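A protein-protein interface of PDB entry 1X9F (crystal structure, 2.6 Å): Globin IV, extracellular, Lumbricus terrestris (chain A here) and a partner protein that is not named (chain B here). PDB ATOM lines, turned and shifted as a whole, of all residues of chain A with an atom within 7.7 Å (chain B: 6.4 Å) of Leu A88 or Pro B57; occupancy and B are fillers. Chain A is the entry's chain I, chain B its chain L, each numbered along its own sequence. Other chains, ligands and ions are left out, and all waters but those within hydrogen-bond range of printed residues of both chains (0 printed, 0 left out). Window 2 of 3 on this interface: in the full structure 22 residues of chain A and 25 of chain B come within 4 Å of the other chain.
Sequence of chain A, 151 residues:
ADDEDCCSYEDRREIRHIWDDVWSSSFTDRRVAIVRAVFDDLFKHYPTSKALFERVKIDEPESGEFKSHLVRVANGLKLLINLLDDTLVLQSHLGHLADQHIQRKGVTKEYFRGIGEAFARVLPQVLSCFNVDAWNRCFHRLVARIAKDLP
The guanidinium group (NE) of Arg B50 lies within salt-bridge range of the side-chain carboxylate (OE1) of Glu B58 (3.9 Å). OG of Ser B56 sits close to OE1 of Glu B58 (3.5 Å).
O of Leu A88 touches CB of Pro B57, 3.6 Å away. N of Val A89 touches CB of Pro B57, at 3.9 Å. Val A89 touches Gly B60. CG1 of Val A89 touches N of Ala B61, 3.4 Å away. Pro B57 touches Ser A92 (O to OG, 3.9 Å). Ser A92 touches Glu B58. OG of Ser A92 touches CB of Ala B61, at 3.7 Å. N of His A93 touches CB of Ala B61 (3.8 Å).
Leu A88 touches just one residue of chain B: Pro B57. Pro B57 touches three residues of chain A. Of the printed residues of chain A, Glu B58 touches Ser A92 (3.5 Å). Of the printed residues of chain B, His A93 touches Ala B61. Printed residues of chain B within 4 Å of Ser A92: Pro B57, Glu B58 and Ala B61. The nearest residue of chain B that does not touch Leu A88 is Glu B58 (5.8 Å).
Of the 11 printed residues of chain B, 4 touch a printed residue of chain A. Of the 11 printed residues of chain A, 4 touch a printed residue of chain B. Hydrophobic or aromatic side chains of chain A within 4 Å of the printed part of chain B: Leu A88, Val A89 and His A93. Along chain A the printed residues that touch a printed residue of chain B span positions 88 to 93.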
ATOM      1  N   LEU A  83      -3.862  27.583  -1.311  1.00  0.00           N
ATOM      2  CA  LEU A  83      -2.681  27.603  -2.155  1.00  0.00           C
ATOM      3  C   LEU A  83      -1.645  28.566  -1.603  1.00  0.00           C
ATOM      4  O   LEU A  83      -0.529  28.645  -2.121  1.00  0.00           O
ATOM      5  CB  LEU A  83      -3.059  28.003  -3.582  1.00  0.00           C
ATOM      6  CG  LEU A  83      -2.937  26.990  -4.727  1.00  0.00           C
ATOM      7  CD1 LEU A  83      -3.080  25.538  -4.272  1.00  0.00           C
ATOM      8  CD2 LEU A  83      -3.949  27.327  -5.818  1.00  0.00           C
ATOM      9  N   ASP A  85       0.367  28.445   0.507  1.00  0.00           N
ATOM     10  CA  ASP A  85       1.597  27.798   0.940  1.00  0.00           C
ATOM     11  C   ASP A  85       2.241  26.977  -0.174  1.00  0.00           C
ATOM     12  O   ASP A  85       3.250  26.296   0.045  1.00  0.00           O
ATOM     13  CB  ASP A  85       1.285  26.898   2.125  1.00  0.00           C
ATOM     14  CG  ASP A  85       2.328  26.977   3.200  1.00  0.00           C
ATOM     15  OD1 ASP A  85       2.063  26.455   4.302  1.00  0.00           O
ATOM     16  OD2 ASP A  85       3.437  27.539   3.055  1.00  0.00           O
ATOM     17  N   ASP A  86       1.632  27.023  -1.355  1.00  0.00           N
ATOM     18  CA  ASP A  86       2.179  26.409  -2.554  1.00  0.00           C
ATOM     19  C   ASP A  86       2.257  27.500  -3.609  1.00  0.00           C
ATOM     20  O   ASP A  86       1.499  27.509  -4.586  1.00  0.00           O
ATOM     21  CB  ASP A  86       1.306  25.243  -3.011  1.00  0.00           C
ATOM     22  CG  ASP A  86       1.607  23.967  -2.257  1.00  0.00           C
ATOM     23  OD1 ASP A  86       0.936  23.710  -1.236  1.00  0.00           O
ATOM     24  OD2 ASP A  86       2.503  23.163  -2.601  1.00  0.00           O
ATOM     25  N   THR A  87       3.197  28.415  -3.383  1.00  0.00           N
ATOM     26  CA  THR A  87       3.256  29.700  -4.082  1.00  0.00           C
ATOM     27  C   THR A  87       3.420  29.619  -5.588  1.00  0.00           C
ATOM     28  O   THR A  87       2.918  30.492  -6.298  1.00  0.00           O
ATOM     29  CB  THR A  87       4.357  30.606  -3.504  1.00  0.00           C
ATOM     30  OG1 THR A  87       5.603  29.902  -3.496  1.00  0.00           O
ATOM     31  CG2 THR A  87       4.099  30.911  -2.033  1.00  0.00           C
ATOM     32  N   LEU A  88       4.123  28.604  -6.085  1.00  0.00           N
ATOM     33  CA  LEU A  88       4.248  28.451  -7.533  1.00  0.00           C
ATOM     34  C   LEU A  88       2.948  27.982  -8.164  1.00  0.00           C
ATOM     35  O   LEU A  88       2.561  28.483  -9.224  1.00  0.00           O
ATOM     36  CB  LEU A  88       5.394  27.515  -7.924  1.00  0.00           C
ATOM     37  CG  LEU A  88       6.832  28.005  -7.731  1.00  0.00           C
ATOM     38  CD1 LEU A  88       7.800  26.913  -8.177  1.00  0.00           C
ATOM     39  CD2 LEU A  88       7.108  29.312  -8.476  1.00  0.00           C
ATOM     40  N   VAL A  89       2.280  27.022  -7.525  1.00  0.00           N
ATOM     41  CA  VAL A  89       0.957  26.605  -7.978  1.00  0.00           C
ATOM     42  C   VAL A  89       0.036  27.824  -7.930  1.00  0.00           C
ATOM     43  O   VAL A  89      -0.728  28.066  -8.871  1.00  0.00           O
ATOM     44  CB  VAL A  89       0.370  25.454  -7.115  1.00  0.00           C
ATOM     45  CG1 VAL A  89      -1.032  25.093  -7.572  1.00  0.00           C
ATOM     46  CG2 VAL A  89       1.263  24.222  -7.161  1.00  0.00           C
ATOM     47  N   LEU A  90       0.129  28.588  -6.836  1.00  0.00           N
ATOM     48  CA  LEU A  90      -0.704  29.777  -6.616  1.00  0.00           C
ATOM     49  C   LEU A  90      -0.565  30.771  -7.756  1.00  0.00           C
ATOM     50  O   LEU A  90      -1.559  31.252  -8.295  1.00  0.00           O
ATOM     51  CB  LEU A  90      -0.358  30.466  -5.284  1.00  0.00           C
ATOM     52  CG  LEU A  90      -1.027  31.836  -5.028  1.00  0.00           C
ATOM     53  CD1 LEU A  90      -2.542  31.685  -4.852  1.00  0.00           C
ATOM     54  CD2 LEU A  90      -0.415  32.547  -3.809  1.00  0.00           C
ATOM     55  N   GLN A  91       0.680  31.069  -8.105  1.00  0.00           N
ATOM     56  CA  GLN A  91       1.026  31.980  -9.185  1.00  0.00           C
ATOM     57  C   GLN A  91       0.353  31.556 -10.493  1.00  0.00           C
ATOM     58  O   GLN A  91      -0.334  32.354 -11.138  1.00  0.00           O
ATOM     59  CB  GLN A  91       2.549  31.977  -9.325  1.00  0.00           C
ATOM     60  CG  GLN A  91       3.153  33.049 -10.205  1.00  0.00           C
ATOM     61  CD  GLN A  91       4.680  32.987 -10.198  1.00  0.00           C
ATOM     62  OE1 GLN A  91       5.316  33.244  -9.169  1.00  0.00           O
ATOM     63  NE2 GLN A  91       5.262  32.651 -11.343  1.00  0.00           N
ATOM     64  N   SER A  92       0.540  30.289 -10.858  1.00  0.00           N
ATOM     65  CA  SER A  92      -0.064  29.728 -12.056  1.00  0.00           C
ATOM     66  C   SER A  92      -1.574  29.880 -12.018  1.00  0.00           C
ATOM     67  O   SER A  92      -2.154  30.489 -12.914  1.00  0.00           O
ATOM     68  CB  SER A  92       0.313  28.258 -12.213  1.00  0.00           C
ATOM     69  OG  SER A  92      -0.418  27.671 -13.274  1.00  0.00           O
ATOM     70  N   HIS A  93      -2.202  29.355 -10.971  1.00  0.00           N
ATOM     71  CA  HIS A  93      -3.652  29.398 -10.872  1.00  0.00           C
ATOM     72  C   HIS A  93      -4.260  30.806 -10.915  1.00  0.00           C
ATOM     73  O   HIS A  93      -5.336  31.006 -11.478  1.00  0.00           O
ATOM     74  CB  HIS A  93      -4.145  28.707  -9.611  1.00  0.00           C
ATOM     75  CG  HIS A  93      -5.610  28.882  -9.412  1.00  0.00           C
ATOM     76  ND1 HIS A  93      -6.531  28.364 -10.294  1.00  0.00           N
ATOM     77  CD2 HIS A  93      -6.317  29.584  -8.497  1.00  0.00           C
ATOM     78  CE1 HIS A  93      -7.746  28.706  -9.914  1.00  0.00           C
ATOM     79  NE2 HIS A  93      -7.646  29.448  -8.825  1.00  0.00           N
ATOM     80  N   LEU A  94      -3.576  31.765 -10.299  1.00  0.00           N
ATOM     81  CA  LEU A  94      -4.039  33.146 -10.248  1.00  0.00           C
ATOM     82  C   LEU A  94      -4.239  33.692 -11.669  1.00  0.00           C
ATOM     83  O   LEU A  94      -5.189  34.436 -11.928  1.00  0.00           O
ATOM     84  CB  LEU A  94      -3.008  33.981  -9.487  1.00  0.00           C
ATOM     85  CG  LEU A  94      -3.332  34.802  -8.231  1.00  0.00           C
ATOM     86  CD1 LEU A  94      -4.509  34.289  -7.429  1.00  0.00           C
ATOM     87  CD2 LEU A  94      -2.095  34.875  -7.353  1.00  0.00           C
ATOM     88  N   ARG B  50      -0.060  21.116 -18.940  1.00  0.00           N
ATOM     89  CA  ARG B  50       1.152  20.312 -18.745  1.00  0.00           C
ATOM     90  C   ARG B  50       0.866  18.939 -18.128  1.00  0.00           C
ATOM     91  O   ARG B  50       1.379  18.601 -17.058  1.00  0.00           O
ATOM     92  CB  ARG B  50       2.207  21.091 -17.947  1.00  0.00           C
ATOM     93  CG  ARG B  50       2.686  22.331 -18.676  1.00  0.00           C
ATOM     94  CD  ARG B  50       3.980  22.946 -18.154  1.00  0.00           C
ATOM     95  NE  ARG B  50       5.097  22.000 -17.980  1.00  0.00           N
ATOM     96  CZ  ARG B  50       5.637  21.245 -18.948  1.00  0.00           C
ATOM     97  NH1 ARG B  50       5.162  21.272 -20.202  1.00  0.00           N
ATOM     98  NH2 ARG B  50       6.656  20.443 -18.654  1.00  0.00           N
ATOM     99  N   ASN B  53       3.795  16.674 -17.433  1.00  0.00           N
ATOM    100  CA  ASN B  53       4.521  16.869 -16.189  1.00  0.00           C
ATOM    101  C   ASN B  53       3.571  17.204 -15.038  1.00  0.00           C
ATOM    102  O   ASN B  53       3.266  18.378 -14.798  1.00  0.00           O
ATOM    103  CB  ASN B  53       5.578  17.967 -16.348  1.00  0.00           C
ATOM    104  CG  ASN B  53       6.437  18.125 -15.110  1.00  0.00           C
ATOM    105  OD1 ASN B  53       6.142  17.565 -14.051  1.00  0.00           O
ATOM    106  ND2 ASN B  53       7.514  18.890 -15.235  1.00  0.00           N
ATOM    107  N   ILE B  54       3.111  16.180 -14.322  1.00  0.00           N
ATOM    108  CA  ILE B  54       2.136  16.393 -13.247  1.00  0.00           C
ATOM    109  C   ILE B  54       2.742  17.089 -12.026  1.00  0.00           C
ATOM    110  O   ILE B  54       2.010  17.519 -11.134  1.00  0.00           O
ATOM    111  CB  ILE B  54       1.430  15.073 -12.831  1.00  0.00           C
ATOM    112  CG1 ILE B  54       2.458  14.027 -12.404  1.00  0.00           C
ATOM    113  CG2 ILE B  54       0.554  14.565 -13.986  1.00  0.00           C
ATOM    114  CD1 ILE B  54       1.874  12.852 -11.684  1.00  0.00           C
ATOM    115  N   TYR B  55       4.065  17.201 -11.988  1.00  0.00           N
ATOM    116  CA  TYR B  55       4.736  17.840 -10.861  1.00  0.00           C
ATOM    117  C   TYR B  55       4.965  19.322 -11.118  1.00  0.00           C
ATOM    118  O   TYR B  55       5.510  20.024 -10.268  1.00  0.00           O
ATOM    119  CB  TYR B  55       6.067  17.144 -10.560  1.00  0.00           C
ATOM    120  CG  TYR B  55       5.917  15.713 -10.102  1.00  0.00           C
ATOM    121  CD1 TYR B  55       5.802  14.673 -11.027  1.00  0.00           C
ATOM    122  CD2 TYR B  55       5.893  15.391  -8.743  1.00  0.00           C
ATOM    123  CE1 TYR B  55       5.657  13.343 -10.610  1.00  0.00           C
ATOM    124  CE2 TYR B  55       5.752  14.063  -8.315  1.00  0.00           C
ATOM    125  CZ  TYR B  55       5.633  13.046  -9.256  1.00  0.00           C
ATOM    126  OH  TYR B  55       5.493  11.736  -8.848  1.00  0.00           O
ATOM    127  N   SER B  56       4.550  19.795 -12.290  1.00  0.00           N
ATOM    128  CA  SER B  56       4.708  21.200 -12.659  1.00  0.00           C
ATOM    129  C   SER B  56       3.662  22.064 -11.942  1.00  0.00           C
ATOM    130  O   SER B  56       2.599  21.554 -11.575  1.00  0.00           O
ATOM    131  CB  SER B  56       4.587  21.358 -14.177  1.00  0.00           C
ATOM    132  OG  SER B  56       3.235  21.189 -14.587  1.00  0.00           O
ATOM    133  N   PRO B  57       3.934  23.355 -11.736  1.00  0.00           N
ATOM    134  CA  PRO B  57       2.955  24.203 -11.063  1.00  0.00           C
ATOM    135  C   PRO B  57       1.676  24.365 -11.897  1.00  0.00           C
ATOM    136  O   PRO B  57       0.589  24.478 -11.329  1.00  0.00           O
ATOM    137  CB  PRO B  57       3.696  25.534 -10.874  1.00  0.00           C
ATOM    138  CG  PRO B  57       4.735  25.541 -11.949  1.00  0.00           C
ATOM    139  CD  PRO B  57       5.146  24.107 -12.120  1.00  0.00           C
ATOM    140  N   GLU B  58       1.806  24.345 -13.224  1.00  0.00           N
ATOM    141  CA  GLU B  58       0.643  24.429 -14.124  1.00  0.00           C
ATOM    142  C   GLU B  58      -0.359  23.285 -13.937  1.00  0.00           C
ATOM    143  O   GLU B  58      -1.570  23.526 -13.869  1.00  0.00           O
ATOM    144  CB  GLU B  58       1.069  24.490 -15.595  1.00  0.00           C
ATOM    145  CG  GLU B  58       1.861  25.726 -15.991  1.00  0.00           C
ATOM    146  CD  GLU B  58       3.305  25.670 -15.532  1.00  0.00           C
ATOM    147  OE1 GLU B  58       3.836  24.558 -15.319  1.00  0.00           O
ATOM    148  OE2 GLU B  58       3.913  26.749 -15.376  1.00  0.00           O
ATOM    149  N   PHE B  59       0.140  22.047 -13.871  1.00  0.00           N
ATOM    150  CA  PHE B  59      -0.741  20.900 -13.637  1.00  0.00           C
ATOM    151  C   PHE B  59      -1.266  20.888 -12.207  1.00  0.00           C
ATOM    152  O   PHE B  59      -2.397  20.461 -11.958  1.00  0.00           O
ATOM    153  CB  PHE B  59      -0.084  19.549 -13.974  1.00  0.00           C
ATOM    154  CG  PHE B  59      -1.058  18.392 -13.924  1.00  0.00           C
ATOM    155  CD1 PHE B  59      -1.857  18.090 -15.024  1.00  0.00           C
ATOM    156  CD2 PHE B  59      -1.215  17.643 -12.757  1.00  0.00           C
ATOM    157  CE1 PHE B  59      -2.778  17.047 -14.972  1.00  0.00           C
ATOM    158  CE2 PHE B  59      -2.137  16.598 -12.694  1.00  0.00           C
ATOM    159  CZ  PHE B  59      -2.919  16.298 -13.802  1.00  0.00           C
ATOM    160  N   GLY B  60      -0.431  21.354 -11.281  1.00  0.00           N
ATOM    161  CA  GLY B  60      -0.802  21.444  -9.875  1.00  0.00           C
ATOM    162  C   GLY B  60      -2.010  22.337  -9.724  1.00  0.00           C
ATOM    163  O   GLY B  60      -2.949  22.005  -8.997  1.00  0.00           O
ATOM    164  N   ALA B  61      -1.982  23.467 -10.431  1.00  0.00           N
ATOM    165  CA  ALA B  61      -3.108  24.395 -10.488  1.00  0.00           C
ATOM    166  C   ALA B  61      -4.368  23.704 -11.008  1.00  0.00           C
ATOM    167  O   ALA B  61      -5.422  23.757 -10.363  1.00  0.00           O
ATOM    168  CB  ALA B  61      -2.761  25.604 -11.352  1.00  0.00           C
ATOM    169  N   HIS B  62      -4.251  23.051 -12.164  1.00  0.00           N
ATOM    170  CA  HIS B  62      -5.365  22.306 -12.736  1.00  0.00           C
ATOM    171  C   HIS B  62      -5.895  21.290 -11.729  1.00  0.00           C
ATOM    172  O   HIS B  62      -7.096  21.232 -11.457  1.00  0.00           O
ATOM    173  CB  HIS B  62      -4.952  21.585 -14.018  1.00  0.00           C
ATOM    174  CG  HIS B  62      -5.939  20.552 -14.447  1.00  0.00           C
ATOM    175  ND1 HIS B  62      -7.179  20.887 -14.945  1.00  0.00           N
ATOM    176  CD2 HIS B  62      -5.907  19.201 -14.384  1.00  0.00           C
ATOM    177  CE1 HIS B  62      -7.851  19.785 -15.213  1.00  0.00           C
ATOM    178  NE2 HIS B  62      -7.106  18.747 -14.873  1.00  0.00           N
